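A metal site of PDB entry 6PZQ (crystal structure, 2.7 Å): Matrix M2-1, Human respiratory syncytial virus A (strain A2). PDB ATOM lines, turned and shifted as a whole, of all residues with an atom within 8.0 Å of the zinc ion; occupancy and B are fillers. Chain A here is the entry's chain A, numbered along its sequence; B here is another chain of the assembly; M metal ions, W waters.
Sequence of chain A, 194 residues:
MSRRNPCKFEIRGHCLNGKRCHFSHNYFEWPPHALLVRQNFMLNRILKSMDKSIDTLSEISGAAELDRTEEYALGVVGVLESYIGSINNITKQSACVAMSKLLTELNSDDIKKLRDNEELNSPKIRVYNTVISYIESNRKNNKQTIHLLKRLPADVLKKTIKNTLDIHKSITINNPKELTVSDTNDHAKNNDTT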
ATOM      1  N   PRO A   6      19.279 -26.169  20.670  1.00  0.00           N
ATOM      2  CA  PRO A   6      19.155 -25.821  22.084  1.00  0.00           C
ATOM      3  C   PRO A   6      17.728 -25.796  22.558  1.00  0.00           C
ATOM      4  O   PRO A   6      16.840 -25.233  21.922  1.00  0.00           O
ATOM      5  CB  PRO A   6      19.773 -24.422  22.167  1.00  0.00           C
ATOM      6  CG  PRO A   6      20.500 -24.241  21.008  1.00  0.00           C
ATOM      7  CD  PRO A   6      20.096 -25.178  19.953  1.00  0.00           C
ATOM      8  N   CYS A   7      17.535 -26.376  23.730  1.00  0.00           N
ATOM      9  CA  CYS A   7      16.259 -26.198  24.419  1.00  0.00           C
ATOM     10  C   CYS A   7      15.986 -24.719  24.583  1.00  0.00           C
ATOM     11  O   CYS A   7      16.735 -24.061  25.313  1.00  0.00           O
ATOM     12  CB  CYS A   7      16.310 -26.841  25.763  1.00  0.00           C
ATOM     13  SG  CYS A   7      14.793 -26.881  26.580  1.00  0.00           S
ATOM     14  N   LYS A   8      14.937 -24.195  23.929  1.00  0.00           N
ATOM     15  CA  LYS A   8      14.505 -22.799  24.151  1.00  0.00           C
ATOM     16  C   LYS A   8      13.941 -22.546  25.550  1.00  0.00           C
ATOM     17  O   LYS A   8      13.915 -21.393  25.999  1.00  0.00           O
ATOM     18  CB  LYS A   8      13.464 -22.381  23.112  1.00  0.00           C
ATOM     19  CG  LYS A   8      14.062 -21.982  21.738  1.00  0.00           C
ATOM     20  CD  LYS A   8      13.012 -21.461  20.731  1.00  0.00           C
ATOM     21  CE  LYS A   8      13.362 -21.815  19.283  1.00  0.00           C
ATOM     22  NZ  LYS A   8      12.150 -22.325  18.545  1.00  0.00           N
ATOM     23  N   PHE A   9      13.495 -23.563  26.272  1.00  0.00           N
ATOM     24  CA  PHE A   9      13.190 -23.324  27.667  1.00  0.00           C
ATOM     25  C   PHE A   9      14.457 -23.012  28.433  1.00  0.00           C
ATOM     26  O   PHE A   9      14.493 -22.077  29.236  1.00  0.00           O
ATOM     27  CB  PHE A   9      12.447 -24.515  28.262  1.00  0.00           C
ATOM     28  CG  PHE A   9      11.046 -24.625  27.768  1.00  0.00           C
ATOM     29  CD1 PHE A   9      10.032 -23.867  28.359  1.00  0.00           C
ATOM     30  CD2 PHE A   9      10.734 -25.435  26.676  1.00  0.00           C
ATOM     31  CE1 PHE A   9       8.708 -23.917  27.891  1.00  0.00           C
ATOM     32  CE2 PHE A   9       9.414 -25.496  26.189  1.00  0.00           C
ATOM     33  CZ  PHE A   9       8.407 -24.738  26.793  1.00  0.00           C
ATOM     34  N   GLU A  10      15.520 -23.787  28.208  1.00  0.00           N
ATOM     35  CA  GLU A  10      16.781 -23.559  28.917  1.00  0.00           C
ATOM     36  C   GLU A  10      17.403 -22.244  28.509  1.00  0.00           C
ATOM     37  O   GLU A  10      18.044 -21.567  29.334  1.00  0.00           O
ATOM     38  CB  GLU A  10      17.734 -24.716  28.638  1.00  0.00           C
ATOM     39  CG  GLU A  10      19.062 -24.699  29.369  1.00  0.00           C
ATOM     40  CD  GLU A  10      19.025 -25.193  30.814  1.00  0.00           C
ATOM     41  OE1 GLU A  10      18.070 -25.924  31.186  1.00  0.00           O
ATOM     42  OE2 GLU A  10      19.972 -24.846  31.577  1.00  0.00           O
ATOM     43  N   ILE A  11      17.204 -21.823  27.256  1.00  0.00           N
ATOM     44  CA  ILE A  11      17.686 -20.516  26.833  1.00  0.00           C
ATOM     45  C   ILE A  11      17.144 -19.396  27.709  1.00  0.00           C
ATOM     46  O   ILE A  11      17.813 -18.381  27.916  1.00  0.00           O
ATOM     47  CB  ILE A  11      17.310 -20.236  25.388  1.00  0.00           C
ATOM     48  CG1 ILE A  11      18.094 -21.191  24.491  1.00  0.00           C
ATOM     49  CG2 ILE A  11      17.586 -18.765  25.117  1.00  0.00           C
ATOM     50  CD1 ILE A  11      17.966 -20.948  23.009  1.00  0.00           C
ATOM     51  N   HIS A  14      15.914 -22.275  33.043  1.00  0.00           N
ATOM     52  CA  HIS A  14      15.978 -23.699  33.359  1.00  0.00           C
ATOM     53  C   HIS A  14      14.797 -24.443  32.739  1.00  0.00           C
ATOM     54  O   HIS A  14      13.640 -24.020  32.934  1.00  0.00           O
ATOM     55  CB  HIS A  14      15.995 -23.898  34.870  1.00  0.00           C
ATOM     56  CG  HIS A  14      16.313 -25.309  35.282  1.00  0.00           C
ATOM     57  ND1 HIS A  14      17.402 -26.001  34.798  1.00  0.00           N
ATOM     58  CD2 HIS A  14      15.680 -26.165  36.120  1.00  0.00           C
ATOM     59  CE1 HIS A  14      17.430 -27.219  35.328  1.00  0.00           C
ATOM     60  NE2 HIS A  14      16.392 -27.338  36.132  1.00  0.00           N
ATOM     61  N   CYS A  15      15.063 -25.539  32.006  1.00  0.00           N
ATOM     62  CA  CYS A  15      13.987 -26.370  31.462  1.00  0.00           C
ATOM     63  C   CYS A  15      13.317 -27.137  32.564  1.00  0.00           C
ATOM     64  O   CYS A  15      13.991 -27.692  33.423  1.00  0.00           O
ATOM     65  CB  CYS A  15      14.493 -27.389  30.445  1.00  0.00           C
ATOM     66  SG  CYS A  15      13.259 -28.537  29.757  1.00  0.00           S
ATOM     67  N   LEU A  16      11.972 -27.197  32.526  1.00  0.00           N
ATOM     68  CA  LEU A  16      11.188 -27.848  33.548  1.00  0.00           C
ATOM     69  C   LEU A  16      10.490 -29.112  33.062  1.00  0.00           C
ATOM     70  O   LEU A  16       9.674 -29.680  33.811  1.00  0.00           O
ATOM     71  CB  LEU A  16      10.158 -26.870  34.120  1.00  0.00           C
ATOM     72  CG  LEU A  16      10.708 -25.757  35.014  1.00  0.00           C
ATOM     73  CD1 LEU A  16       9.615 -24.826  35.469  1.00  0.00           C
ATOM     74  CD2 LEU A  16      11.435 -26.311  36.187  1.00  0.00           C
ATOM     75  N   ASN A  17      10.801 -29.580  31.840  1.00  0.00           N
ATOM     76  CA  ASN A  17      10.193 -30.763  31.247  1.00  0.00           C
ATOM     77  C   ASN A  17      10.780 -32.070  31.774  1.00  0.00           C
ATOM     78  O   ASN A  17      10.057 -32.916  32.287  1.00  0.00           O
ATOM     79  CB  ASN A  17      10.329 -30.685  29.743  1.00  0.00           C
ATOM     80  CG  ASN A  17       9.210 -29.947  29.117  1.00  0.00           C
ATOM     81  OD1 ASN A  17       9.351 -28.800  28.616  1.00  0.00           O
ATOM     82  ND2 ASN A  17       8.043 -30.587  29.157  1.00  0.00           N
ATOM     83  N   GLY A  18      12.083 -32.257  31.694  1.00  0.00           N
ATOM     84  CA  GLY A  18      12.765 -33.449  32.176  1.00  0.00           C
ATOM     85  C   GLY A  18      13.233 -34.316  31.024  1.00  0.00           C
ATOM     86  O   GLY A  18      13.407 -33.854  29.886  1.00  0.00           O
ATOM     87  N   LYS A  19      13.403 -35.621  31.327  1.00  0.00           N
ATOM     88  CA  LYS A  19      13.836 -36.521  30.272  1.00  0.00           C
ATOM     89  C   LYS A  19      12.893 -36.537  29.062  1.00  0.00           C
ATOM     90  O   LYS A  19      13.249 -37.151  28.059  1.00  0.00           O
ATOM     91  CB  LYS A  19      14.029 -37.932  30.807  1.00  0.00           C
ATOM     92  CG  LYS A  19      12.699 -38.770  30.994  1.00  0.00           C
ATOM     93  CD  LYS A  19      12.352 -39.824  29.839  1.00  0.00           C
ATOM     94  CE  LYS A  19      11.180 -40.769  30.252  1.00  0.00           C
ATOM     95  NZ  LYS A  19      10.475 -41.488  29.082  1.00  0.00           N
ATOM     96  N   ARG A  20      11.718 -35.882  29.121  1.00  0.00           N
ATOM     97  CA  ARG A  20      10.840 -35.737  27.937  1.00  0.00           C
ATOM     98  C   ARG A  20      11.379 -34.763  26.901  1.00  0.00           C
ATOM     99  O   ARG A  20      11.006 -34.886  25.723  1.00  0.00           O
ATOM    100  CB  ARG A  20       9.429 -35.258  28.310  1.00  0.00           C
ATOM    101  CG  ARG A  20       8.755 -36.044  29.423  1.00  0.00           C
ATOM    102  CD  ARG A  20       7.894 -35.157  30.336  1.00  0.00           C
ATOM    103  NE  ARG A  20       6.509 -35.173  29.901  1.00  0.00           N
ATOM    104  CZ  ARG A  20       5.669 -34.169  30.023  1.00  0.00           C
ATOM    105  NH1 ARG A  20       6.093 -33.046  30.572  1.00  0.00           N
ATOM    106  NH2 ARG A  20       4.419 -34.298  29.590  1.00  0.00           N
ATOM    107  N   CYS A  21      12.213 -33.779  27.267  1.00  0.00           N
ATOM    108  CA  CYS A  21      12.667 -32.778  26.319  1.00  0.00           C
ATOM    109  C   CYS A  21      13.884 -33.336  25.622  1.00  0.00           C
ATOM    110  O   CYS A  21      14.882 -33.689  26.272  1.00  0.00           O
ATOM    111  CB  CYS A  21      12.963 -31.424  26.995  1.00  0.00           C
ATOM    112  SG  CYS A  21      13.731 -30.134  25.798  1.00  0.00           S
ATOM    113  N   HIS A  22      13.796 -33.453  24.301  1.00  0.00           N
ATOM    114  CA  HIS A  22      14.836 -34.018  23.454  1.00  0.00           C
ATOM    115  C   HIS A  22      15.662 -32.934  22.785  1.00  0.00           C
ATOM    116  O   HIS A  22      16.127 -33.088  21.643  1.00  0.00           O
ATOM    117  CB  HIS A  22      14.184 -34.928  22.436  1.00  0.00           C
ATOM    118  CG  HIS A  22      13.352 -35.983  23.091  1.00  0.00           C
ATOM    119  ND1 HIS A  22      12.060 -36.259  22.699  1.00  0.00           N
ATOM    120  CD2 HIS A  22      13.625 -36.789  24.142  1.00  0.00           C
ATOM    121  CE1 HIS A  22      11.577 -37.221  23.480  1.00  0.00           C
ATOM    122  NE2 HIS A  22      12.504 -37.558  24.359  1.00  0.00           N
ATOM    123  N   PHE A  23      15.843 -31.819  23.468  1.00  0.00           N
ATOM    124  CA  PHE A  23      16.719 -30.762  23.000  1.00  0.00           C
ATOM    125  C   PHE A  23      17.884 -30.616  23.959  1.00  0.00           C
ATOM    126  O   PHE A  23      17.865 -31.101  25.097  1.00  0.00           O
ATOM    127  CB  PHE A  23      15.957 -29.465  22.863  1.00  0.00           C
ATOM    128  CG  PHE A  23      14.806 -29.542  21.893  1.00  0.00           C
ATOM    129  CD1 PHE A  23      13.576 -30.016  22.288  1.00  0.00           C
ATOM    130  CD2 PHE A  23      14.967 -29.132  20.569  1.00  0.00           C
ATOM    131  CE1 PHE A  23      12.519 -30.079  21.393  1.00  0.00           C
ATOM    132  CE2 PHE A  23      13.914 -29.206  19.655  1.00  0.00           C
ATOM    133  CZ  PHE A  23      12.701 -29.670  20.065  1.00  0.00           C
ATOM    134  N   SER A  24      18.897 -29.943  23.482  1.00  0.00           N
ATOM    135  CA  SER A  24      20.137 -29.813  24.233  1.00  0.00           C
ATOM    136  C   SER A  24      20.010 -28.906  25.462  1.00  0.00           C
ATOM    137  O   SER A  24      19.590 -27.753  25.362  1.00  0.00           O
ATOM    138  CB  SER A  24      21.219 -29.259  23.338  1.00  0.00           C
ATOM    139  OG  SER A  24      22.366 -29.242  24.166  1.00  0.00           O
ATOM    140  N   HIS A  25      20.337 -29.455  26.623  1.00  0.00           N
ATOM    141  CA  HIS A  25      20.651 -28.718  27.824  1.00  0.00           C
ATOM    142  C   HIS A  25      22.148 -28.751  28.147  1.00  0.00           C
ATOM    143  O   HIS A  25      22.554 -28.491  29.281  1.00  0.00           O
ATOM    144  CB  HIS A  25      19.794 -29.279  28.966  1.00  0.00           C
ATOM    145  CG  HIS A  25      18.377 -29.495  28.537  1.00  0.00           C
ATOM    146  ND1 HIS A  25      17.768 -30.735  28.579  1.00  0.00           N
ATOM    147  CD2 HIS A  25      17.480 -28.656  27.972  1.00  0.00           C
ATOM    148  CE1 HIS A  25      16.555 -30.639  28.078  1.00  0.00           C
ATOM    149  NE2 HIS A  25      16.354 -29.388  27.697  1.00  0.00           N
ATOM    150  N   TRP A  30      25.882 -26.023  22.216  1.00  0.00           N
ATOM    151  CA  TRP A  30      25.037 -24.974  21.650  1.00  0.00           C
ATOM    152  C   TRP A  30      25.826 -24.077  20.726  1.00  0.00           C
ATOM    153  O   TRP A  30      27.030 -23.937  20.866  1.00  0.00           O
ATOM    154  CB  TRP A  30      24.426 -24.101  22.712  1.00  0.00           C
ATOM    155  CG  TRP A  30      23.452 -24.715  23.630  1.00  0.00           C
ATOM    156  CD1 TRP A  30      23.187 -26.034  23.779  1.00  0.00           C
ATOM    157  CD2 TRP A  30      22.629 -24.018  24.556  1.00  0.00           C
ATOM    158  NE1 TRP A  30      22.253 -26.202  24.779  1.00  0.00           N
ATOM    159  CE2 TRP A  30      21.881 -24.972  25.247  1.00  0.00           C
ATOM    160  CE3 TRP A  30      22.455 -22.681  24.861  1.00  0.00           C
ATOM    161  CZ2 TRP A  30      20.967 -24.619  26.246  1.00  0.00           C
ATOM    162  CZ3 TRP A  30      21.539 -22.331  25.828  1.00  0.00           C
ATOM    163  CH2 TRP A  30      20.815 -23.296  26.505  1.00  0.00           C
ATOM    164  P     A B   6       7.053 -30.605  19.095  1.00  0.00           P
ATOM    165  OP1   A B   6       7.368 -30.784  20.537  1.00  0.00           O
ATOM    166  OP2   A B   6       5.674 -30.468  18.557  1.00  0.00           O
ATOM    167  O5'   A B   6       7.805 -29.318  18.589  1.00  0.00           O
ATOM    168  C5'   A B   6       7.340 -28.573  17.481  1.00  0.00           C
ATOM    169  C4'   A B   6       8.291 -27.450  17.277  1.00  0.00           C
ATOM    170  O4'   A B   6       8.383 -26.697  18.501  1.00  0.00           O
ATOM    171  C3'   A B   6       9.696 -27.942  17.007  1.00  0.00           C
ATOM    172  O3'   A B   6       9.935 -28.018  15.625  1.00  0.00           O
ATOM    173  C2'   A B   6      10.611 -26.938  17.694  1.00  0.00           C
ATOM    174  O2'   A B   6      10.985 -25.891  16.815  1.00  0.00           O
ATOM    175  C1'   A B   6       9.721 -26.378  18.799  1.00  0.00           C
ATOM    176  N9    A B   6      10.059 -26.834  20.153  1.00  0.00           N
ATOM    177  C8    A B   6       9.278 -27.481  21.082  1.00  0.00           C
ATOM    178  N7    A B   6       9.878 -27.664  22.227  1.00  0.00           N
ATOM    179  C5    A B   6      11.129 -27.077  22.026  1.00  0.00           C
ATOM    180  C6    A B   6      12.239 -26.938  22.878  1.00  0.00           C
ATOM    181  N6    A B   6      12.275 -27.396  24.122  1.00  0.00           N
ATOM    182  N1    A B   6      13.330 -26.300  22.341  1.00  0.00           N
ATOM    183  C2    A B   6      13.331 -25.804  21.073  1.00  0.00           C
ATOM    184  N3    A B   6      12.346 -25.888  20.178  1.00  0.00           N
ATOM    185  C4    A B   6      11.269 -26.554  20.741  1.00  0.00           C
HETATM  186 ZN    ZN M   1      14.392 -28.607  27.801  1.00  0.00          ZN
HETATM  187  O   HOH W   1      14.852 -30.458  30.354  1.00  0.00           O
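The zinc ion is bound by NE2 of His 25, SG of Cys 7, SG of Cys 15 and SG of Cys 21. The zinc ion has four donor atoms within binding distance.
Of the 20 residues printed, 4 come within 4 Å of the zinc ion. The nearest printed residue that does not touch the zinc ion is A 6 of chain B (4.4 Å).
A ring nitrogen (NE2) of His 25 sits close to the backbone carbonyl oxygen of Phe 23 (3.5 Å). SG of Cys 7 sits close to N6 of A 6 of chain B. The side-chain sulfur (SG) of Cys 7 lies close to the backbone NH (N) of Phe 9. The backbone NH (N) of Cys 7 is in hydrogen-bond range of the backbone carbonyl oxygen (O) of Ser 24 (3.0 Å). N of Asn 17 lies close to SG of Cys 15 (3.4 Å). The backbone NH of Cys 15 is in hydrogen-bond range of the side-chain carboxylate of Glu 10, at 3.1 Å. The side-chain sulfur of Cys 21 lies close to N6 of A 6 of chain B (3.5 Å). SG of Cys 21 sits close to N of Phe 23 (3.6 Å).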
